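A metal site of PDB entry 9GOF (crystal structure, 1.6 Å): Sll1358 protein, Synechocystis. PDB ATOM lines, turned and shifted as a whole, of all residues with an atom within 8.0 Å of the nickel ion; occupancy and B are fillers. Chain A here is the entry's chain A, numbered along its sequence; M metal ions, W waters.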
ATOM      1  N   MET A  57     -36.957 -12.402  33.689  1.00  0.00           N
ATOM      2  CA  MET A  57     -36.263 -13.088  34.785  1.00  0.00           C
ATOM      3  C   MET A  57     -36.419 -12.300  36.075  1.00  0.00           C
ATOM      4  O   MET A  57     -36.473 -11.062  36.054  1.00  0.00           O
ATOM      5  CB  MET A  57     -34.781 -13.329  34.425  1.00  0.00           C
ATOM      6  CG  MET A  57     -33.916 -13.872  35.561  1.00  0.00           C
ATOM      7  SD  MET A  57     -32.273 -14.346  34.920  1.00  0.00           S
ATOM      8  CE  MET A  57     -32.731 -15.743  33.896  1.00  0.00           C
ATOM      9  N   ARG A  65     -27.802 -15.200  38.967  1.00  0.00           N
ATOM     10  CA  ARG A  65     -27.703 -15.868  37.675  1.00  0.00           C
ATOM     11  C   ARG A  65     -26.219 -16.072  37.429  1.00  0.00           C
ATOM     12  O   ARG A  65     -25.475 -15.103  37.263  1.00  0.00           O
ATOM     13  CB  ARG A  65     -28.371 -15.010  36.601  1.00  0.00           C
ATOM     14  CG  ARG A  65     -28.231 -15.530  35.165  1.00  0.00           C
ATOM     15  CD  ARG A  65     -29.061 -16.806  34.931  1.00  0.00           C
ATOM     16  NE  ARG A  65     -28.933 -17.238  33.541  1.00  0.00           N
ATOM     17  CZ  ARG A  65     -27.993 -18.069  33.098  1.00  0.00           C
ATOM     18  NH1 ARG A  65     -27.152 -18.670  33.937  1.00  0.00           N
ATOM     19  NH2 ARG A  65     -27.886 -18.302  31.787  1.00  0.00           N
ATOM     20  N   GLU A  66     -25.766 -17.333  37.469  1.00  0.00           N
ATOM     21  CA  GLU A  66     -24.354 -17.652  37.573  1.00  0.00           C
ATOM     22  C   GLU A  66     -23.561 -17.130  36.379  1.00  0.00           C
ATOM     23  O   GLU A  66     -24.111 -16.811  35.323  1.00  0.00           O
ATOM     24  CB  GLU A  66     -24.141 -19.155  37.669  1.00  0.00           C
ATOM     25  CG  GLU A  66     -24.520 -19.891  36.383  1.00  0.00           C
ATOM     26  CD  GLU A  66     -23.919 -21.282  36.280  1.00  0.00           C
ATOM     27  OE1 GLU A  66     -22.861 -21.537  36.889  1.00  0.00           O
ATOM     28  OE2 GLU A  66     -24.540 -22.143  35.608  1.00  0.00           O
ATOM     29  N   LEU A  67     -22.249 -17.093  36.570  1.00  0.00           N
ATOM     30  CA  LEU A  67     -21.327 -16.735  35.506  1.00  0.00           C
ATOM     31  C   LEU A  67     -21.562 -17.586  34.261  1.00  0.00           C
ATOM     32  O   LEU A  67     -21.529 -18.821  34.329  1.00  0.00           O
ATOM     33  CB  LEU A  67     -19.904 -16.915  36.023  1.00  0.00           C
ATOM     34  CG  LEU A  67     -19.469 -15.860  37.048  1.00  0.00           C
ATOM     35  CD1 LEU A  67     -18.231 -16.305  37.830  1.00  0.00           C
ATOM     36  CD2 LEU A  67     -19.214 -14.514  36.366  1.00  0.00           C
ATOM     37  N   HIS A  68     -21.828 -16.937  33.120  1.00  0.00           N
ATOM     38  CA  HIS A  68     -22.086 -17.655  31.883  1.00  0.00           C
ATOM     39  C   HIS A  68     -21.746 -16.741  30.715  1.00  0.00           C
ATOM     40  O   HIS A  68     -21.447 -15.560  30.882  1.00  0.00           O
ATOM     41  CB  HIS A  68     -23.554 -18.133  31.789  1.00  0.00           C
ATOM     42  CG  HIS A  68     -24.544 -17.015  31.605  1.00  0.00           C
ATOM     43  ND1 HIS A  68     -25.068 -16.302  32.663  1.00  0.00           N
ATOM     44  CD2 HIS A  68     -25.094 -16.486  30.483  1.00  0.00           C
ATOM     45  CE1 HIS A  68     -25.898 -15.380  32.195  1.00  0.00           C
ATOM     46  NE2 HIS A  68     -25.932 -15.475  30.883  1.00  0.00           N
ATOM     47  N   TRP A  69     -21.823 -17.296  29.510  1.00  0.00           N
ATOM     48  CA  TRP A  69     -21.631 -16.504  28.294  1.00  0.00           C
ATOM     49  C   TRP A  69     -22.474 -17.094  27.173  1.00  0.00           C
ATOM     50  O   TRP A  69     -22.966 -18.218  27.271  1.00  0.00           O
ATOM     51  CB  TRP A  69     -20.139 -16.419  27.877  1.00  0.00           C
ATOM     52  CG  TRP A  69     -19.540 -17.659  27.207  1.00  0.00           C
ATOM     53  CD1 TRP A  69     -19.453 -17.904  25.869  1.00  0.00           C
ATOM     54  CD2 TRP A  69     -18.919 -18.778  27.860  1.00  0.00           C
ATOM     55  NE1 TRP A  69     -18.827 -19.105  25.642  1.00  0.00           N
ATOM     56  CE2 TRP A  69     -18.485 -19.668  26.845  1.00  0.00           C
ATOM     57  CE3 TRP A  69     -18.687 -19.127  29.201  1.00  0.00           C
ATOM     58  CZ2 TRP A  69     -17.842 -20.873  27.127  1.00  0.00           C
ATOM     59  CZ3 TRP A  69     -18.058 -20.335  29.483  1.00  0.00           C
ATOM     60  CH2 TRP A  69     -17.633 -21.187  28.442  1.00  0.00           C
ATOM     61  N   HIS A  70     -22.650 -16.319  26.109  1.00  0.00           N
ATOM     62  CA  HIS A  70     -23.370 -16.824  24.934  1.00  0.00           C
ATOM     63  C   HIS A  70     -22.892 -16.007  23.735  1.00  0.00           C
ATOM     64  O   HIS A  70     -23.307 -14.864  23.552  1.00  0.00           O
ATOM     65  CB  HIS A  70     -24.894 -16.739  25.108  1.00  0.00           C
ATOM     66  CG  HIS A  70     -25.352 -15.663  26.048  1.00  0.00           C
ATOM     67  ND1 HIS A  70     -25.331 -14.323  25.717  1.00  0.00           N
ATOM     68  CD2 HIS A  70     -25.863 -15.732  27.305  1.00  0.00           C
ATOM     69  CE1 HIS A  70     -25.790 -13.610  26.740  1.00  0.00           C
ATOM     70  NE2 HIS A  70     -26.110 -14.448  27.717  1.00  0.00           N
ATOM     71  N   ALA A  73     -25.428 -14.281  20.900  1.00  0.00           N
ATOM     72  CA  ALA A  73     -26.389 -13.203  21.094  1.00  0.00           C
ATOM     73  C   ALA A  73     -25.830 -12.133  22.024  1.00  0.00           C
ATOM     74  O   ALA A  73     -25.282 -12.444  23.085  1.00  0.00           O
ATOM     75  CB  ALA A  73     -27.707 -13.736  21.673  1.00  0.00           C
ATOM     76  N   ALA A  74     -25.989 -10.870  21.620  1.00  0.00           N
ATOM     77  CA  ALA A  74     -25.849  -9.775  22.561  1.00  0.00           C
ATOM     78  C   ALA A  74     -27.083  -9.717  23.467  1.00  0.00           C
ATOM     79  O   ALA A  74     -28.178 -10.125  23.061  1.00  0.00           O
ATOM     80  CB  ALA A  74     -25.671  -8.447  21.823  1.00  0.00           C
ATOM     81  N   GLU A  75     -26.898  -9.187  24.672  1.00  0.00           N
ATOM     82  CA  GLU A  75     -27.903  -9.188  25.730  1.00  0.00           C
ATOM     83  C   GLU A  75     -28.169  -7.755  26.166  1.00  0.00           C
ATOM     84  O   GLU A  75     -27.288  -7.093  26.726  1.00  0.00           O
ATOM     85  CB  GLU A  75     -27.438 -10.035  26.910  1.00  0.00           C
ATOM     86  CG  GLU A  75     -28.377 -10.043  28.135  1.00  0.00           C
ATOM     87  CD  GLU A  75     -27.905 -11.036  29.169  1.00  0.00           C
ATOM     88  OE1 GLU A  75     -27.437 -12.114  28.751  1.00  0.00           O
ATOM     89  OE2 GLU A  75     -28.002 -10.760  30.396  1.00  0.00           O
ATOM     90  N   TRP A 106     -28.611  -2.711  30.898  1.00  0.00           N
ATOM     91  CA  TRP A 106     -27.248  -3.148  30.601  1.00  0.00           C
ATOM     92  C   TRP A 106     -27.187  -3.701  29.191  1.00  0.00           C
ATOM     93  O   TRP A 106     -28.215  -4.020  28.570  1.00  0.00           O
ATOM     94  CB  TRP A 106     -26.719  -4.167  31.619  1.00  0.00           C
ATOM     95  CG  TRP A 106     -27.415  -5.511  31.729  1.00  0.00           C
ATOM     96  CD1 TRP A 106     -27.308  -6.592  30.888  1.00  0.00           C
ATOM     97  CD2 TRP A 106     -28.271  -5.934  32.802  1.00  0.00           C
ATOM     98  NE1 TRP A 106     -28.041  -7.658  31.384  1.00  0.00           N
ATOM     99  CE2 TRP A 106     -28.646  -7.269  32.548  1.00  0.00           C
ATOM    100  CE3 TRP A 106     -28.752  -5.294  33.951  1.00  0.00           C
ATOM    101  CZ2 TRP A 106     -29.493  -7.976  33.409  1.00  0.00           C
ATOM    102  CZ3 TRP A 106     -29.594  -5.998  34.789  1.00  0.00           C
ATOM    103  CH2 TRP A 106     -29.958  -7.322  34.522  1.00  0.00           C
ATOM    104  N   PHE A 108     -24.584  -6.526  27.287  1.00  0.00           N
ATOM    105  CA  PHE A 108     -23.442  -7.443  27.315  1.00  0.00           C
ATOM    106  C   PHE A 108     -23.112  -7.843  25.885  1.00  0.00           C
ATOM    107  O   PHE A 108     -23.912  -8.550  25.252  1.00  0.00           O
ATOM    108  CB  PHE A 108     -23.782  -8.687  28.131  1.00  0.00           C
ATOM    109  CG  PHE A 108     -24.110  -8.419  29.582  1.00  0.00           C
ATOM    110  CD1 PHE A 108     -23.638  -7.292  30.237  1.00  0.00           C
ATOM    111  CD2 PHE A 108     -24.897  -9.321  30.276  1.00  0.00           C
ATOM    112  CE1 PHE A 108     -23.943  -7.076  31.587  1.00  0.00           C
ATOM    113  CE2 PHE A 108     -25.210  -9.133  31.628  1.00  0.00           C
ATOM    114  CZ  PHE A 108     -24.724  -8.002  32.283  1.00  0.00           C
ATOM    115  N   TRP A 112     -19.206 -12.103  25.768  1.00  0.00           N
ATOM    116  CA  TRP A 112     -18.515 -11.660  26.976  1.00  0.00           C
ATOM    117  C   TRP A 112     -19.123 -12.348  28.191  1.00  0.00           C
ATOM    118  O   TRP A 112     -20.336 -12.559  28.254  1.00  0.00           O
ATOM    119  CB  TRP A 112     -18.599 -10.141  27.127  1.00  0.00           C
ATOM    120  CG  TRP A 112     -17.886  -9.318  26.074  1.00  0.00           C
ATOM    121  CD1 TRP A 112     -17.469  -9.722  24.834  1.00  0.00           C
ATOM    122  CD2 TRP A 112     -17.518  -7.939  26.181  1.00  0.00           C
ATOM    123  NE1 TRP A 112     -16.855  -8.670  24.167  1.00  0.00           N
ATOM    124  CE2 TRP A 112     -16.895  -7.567  24.976  1.00  0.00           C
ATOM    125  CE3 TRP A 112     -17.674  -6.973  27.187  1.00  0.00           C
ATOM    126  CZ2 TRP A 112     -16.410  -6.271  24.757  1.00  0.00           C
ATOM    127  CZ3 TRP A 112     -17.192  -5.690  26.969  1.00  0.00           C
ATOM    128  CH2 TRP A 112     -16.569  -5.348  25.754  1.00  0.00           C
ATOM    129  N   GLY A 113     -18.263 -12.701  29.158  1.00  0.00           N
ATOM    130  CA  GLY A 113     -18.756 -13.388  30.353  1.00  0.00           C
ATOM    131  C   GLY A 113     -19.468 -12.441  31.300  1.00  0.00           C
ATOM    132  O   GLY A 113     -19.126 -11.261  31.427  1.00  0.00           O
ATOM    133  N   HIS A 114     -20.511 -12.955  31.977  1.00  0.00           N
ATOM    134  CA  HIS A 114     -21.276 -12.071  32.854  1.00  0.00           C
ATOM    135  C   HIS A 114     -22.013 -12.848  33.938  1.00  0.00           C
ATOM    136  O   HIS A 114     -22.178 -14.064  33.852  1.00  0.00           O
ATOM    137  CB  HIS A 114     -22.257 -11.202  32.056  1.00  0.00           C
ATOM    138  CG  HIS A 114     -23.141 -11.965  31.122  1.00  0.00           C
ATOM    139  ND1 HIS A 114     -22.732 -12.340  29.851  1.00  0.00           N
ATOM    140  CD2 HIS A 114     -24.434 -12.355  31.233  1.00  0.00           C
ATOM    141  CE1 HIS A 114     -23.727 -12.957  29.238  1.00  0.00           C
ATOM    142  NE2 HIS A 114     -24.775 -12.963  30.042  1.00  0.00           N
ATOM    143  N   SER A 115     -22.452 -12.098  34.946  1.00  0.00           N
ATOM    144  CA  SER A 115     -23.333 -12.603  36.008  1.00  0.00           C
ATOM    145  C   SER A 115     -24.323 -11.502  36.387  1.00  0.00           C
ATOM    146  O   SER A 115     -24.088 -10.328  36.104  1.00  0.00           O
ATOM    147  CB  SER A 115     -22.564 -13.056  37.254  1.00  0.00           C
ATOM    148  OG  SER A 115     -21.984 -11.923  37.919  1.00  0.00           O
ATOM    149  N   ILE A 116     -25.434 -11.888  37.010  1.00  0.00           N
ATOM    150  CA  ILE A 116     -26.452 -10.964  37.488  1.00  0.00           C
ATOM    151  C   ILE A 116     -26.892 -11.415  38.881  1.00  0.00           C
ATOM    152  O   ILE A 116     -27.272 -12.576  39.054  1.00  0.00           O
ATOM    153  CB  ILE A 116     -27.689 -10.892  36.576  1.00  0.00           C
ATOM    154  CG1 ILE A 116     -27.329 -10.734  35.089  1.00  0.00           C
ATOM    155  CG2 ILE A 116     -28.646  -9.794  37.047  1.00  0.00           C
ATOM    156  CD1 ILE A 116     -28.465 -11.285  34.190  1.00  0.00           C
ATOM    157  N   LEU A 128     -34.718  -9.289  29.426  1.00  0.00           N
ATOM    158  CA  LEU A 128     -33.500  -9.422  28.635  1.00  0.00           C
ATOM    159  C   LEU A 128     -33.924  -9.637  27.192  1.00  0.00           C
ATOM    160  O   LEU A 128     -34.794 -10.467  26.922  1.00  0.00           O
ATOM    161  CB  LEU A 128     -32.626 -10.594  29.114  1.00  0.00           C
ATOM    162  CG  LEU A 128     -32.319 -10.680  30.614  1.00  0.00           C
ATOM    163  CD1 LEU A 128     -31.612 -11.997  30.943  1.00  0.00           C
ATOM    164  CD2 LEU A 128     -31.439  -9.532  31.030  1.00  0.00           C
ATOM    165  N   PHE A 130     -32.434 -10.335  23.322  1.00  0.00           N
ATOM    166  CA  PHE A 130     -31.249 -10.871  22.663  1.00  0.00           C
ATOM    167  C   PHE A 130     -31.378 -10.677  21.164  1.00  0.00           C
ATOM    168  O   PHE A 130     -32.447 -10.904  20.595  1.00  0.00           O
ATOM    169  CB  PHE A 130     -31.106 -12.357  22.996  1.00  0.00           C
ATOM    170  CG  PHE A 130     -30.971 -12.615  24.465  1.00  0.00           C
ATOM    171  CD1 PHE A 130     -32.096 -12.724  25.271  1.00  0.00           C
ATOM    172  CD2 PHE A 130     -29.718 -12.710  25.036  1.00  0.00           C
ATOM    173  CE1 PHE A 130     -31.962 -12.930  26.638  1.00  0.00           C
ATOM    174  CE2 PHE A 130     -29.572 -12.935  26.398  1.00  0.00           C
ATOM    175  CZ  PHE A 130     -30.692 -13.038  27.199  1.00  0.00           C
ATOM    176  N   PHE A 135     -32.529 -17.442  20.548  1.00  0.00           N
ATOM    177  CA  PHE A 135     -31.831 -17.522  21.827  1.00  0.00           C
ATOM    178  C   PHE A 135     -32.694 -18.195  22.895  1.00  0.00           C
ATOM    179  O   PHE A 135     -33.880 -17.883  23.030  1.00  0.00           O
ATOM    180  CB  PHE A 135     -31.424 -16.134  22.332  1.00  0.00           C
ATOM    181  CG  PHE A 135     -30.736 -16.192  23.668  1.00  0.00           C
ATOM    182  CD1 PHE A 135     -29.368 -16.420  23.726  1.00  0.00           C
ATOM    183  CD2 PHE A 135     -31.453 -16.101  24.848  1.00  0.00           C
ATOM    184  CE1 PHE A 135     -28.724 -16.524  24.968  1.00  0.00           C
ATOM    185  CE2 PHE A 135     -30.821 -16.187  26.077  1.00  0.00           C
ATOM    186  CZ  PHE A 135     -29.448 -16.401  26.134  1.00  0.00           C
ATOM    187  N   GLU A 137     -32.498 -19.433  27.186  1.00  0.00           N
ATOM    188  CA  GLU A 137     -31.749 -19.486  28.440  1.00  0.00           C
ATOM    189  C   GLU A 137     -31.284 -20.885  28.779  1.00  0.00           C
ATOM    190  O   GLU A 137     -30.407 -21.044  29.633  1.00  0.00           O
ATOM    191  CB  GLU A 137     -32.587 -18.937  29.595  1.00  0.00           C
ATOM    192  CG  GLU A 137     -32.606 -17.430  29.653  1.00  0.00           C
ATOM    193  CD  GLU A 137     -31.364 -16.842  30.299  1.00  0.00           C
ATOM    194  OE1 GLU A 137     -30.716 -17.518  31.134  1.00  0.00           O
ATOM    195  OE2 GLU A 137     -31.018 -15.684  29.946  1.00  0.00           O
ATOM    196  N   THR A 140     -27.207 -21.480  27.315  1.00  0.00           N
ATOM    197  CA  THR A 140     -26.056 -20.640  27.586  1.00  0.00           C
ATOM    198  C   THR A 140     -24.884 -21.505  28.039  1.00  0.00           C
ATOM    199  O   THR A 140     -25.055 -22.662  28.412  1.00  0.00           O
ATOM    200  CB  THR A 140     -26.352 -19.560  28.633  1.00  0.00           C
ATOM    201  OG1 THR A 140     -26.377 -20.121  29.957  1.00  0.00           O
ATOM    202  CG2 THR A 140     -27.674 -18.848  28.314  1.00  0.00           C
ATOM    203  N   PHE A 141     -23.699 -20.921  27.986  1.00  0.00           N
ATOM    204  CA  PHE A 141     -22.482 -21.611  28.385  1.00  0.00           C
ATOM    205  C   PHE A 141     -22.187 -21.274  29.839  1.00  0.00           C
ATOM    206  O   PHE A 141     -21.806 -20.144  30.154  1.00  0.00           O
ATOM    207  CB  PHE A 141     -21.326 -21.209  27.465  1.00  0.00           C
ATOM    208  CG  PHE A 141     -21.402 -21.850  26.110  1.00  0.00           C
ATOM    209  CD1 PHE A 141     -22.362 -21.432  25.199  1.00  0.00           C
ATOM    210  CD2 PHE A 141     -20.558 -22.881  25.764  1.00  0.00           C
ATOM    211  CE1 PHE A 141     -22.464 -22.042  23.958  1.00  0.00           C
ATOM    212  CE2 PHE A 141     -20.650 -23.501  24.523  1.00  0.00           C
ATOM    213  CZ  PHE A 141     -21.598 -23.072  23.617  1.00  0.00           C
HETATM  214 NI    NI M   1     -26.680 -13.846  29.681  1.00  0.00          NI
HETATM  215  O   HOH W   1     -27.554 -13.095  31.420  1.00  0.00           O
HETATM  216  O   HOH W   2     -28.519 -14.877  29.214  1.00  0.00           O
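O of Glu 75 is in hydrogen-bond range of N of Phe 108, 2.8 Å away. The side-chain carboxylate (OE2) of Glu 75 lies within hydrogen-bond range of the indole nitrogen (NE1) of Trp 106, 3.3 Å away. A ring nitrogen (ND1) of His 114 sits at hydrogen-bond distance from the backbone carbonyl oxygen (O) of Trp 112, at 2.9 Å. A ring nitrogen (ND1) of His 70 lies within hydrogen-bond range of the backbone carbonyl oxygen of Ala 73 (3.2 Å). A ring nitrogen (ND1) of His 68 lies within hydrogen-bond range of the guanidinium group (NH1) of Arg 65. O of Glu 66 lies within hydrogen-bond range of ND1 of His 68 (2.9 Å).
The nearest printed residue that does not touch the nickel ion is Phe 130 (4.5 Å).
The nickel ion is bound by water W1, OE1 of Glu 75, NE2 of His 114, NE2 of His 70, NE2 of His 68 and water W2. The nickel ion has six donor atoms within binding distance.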
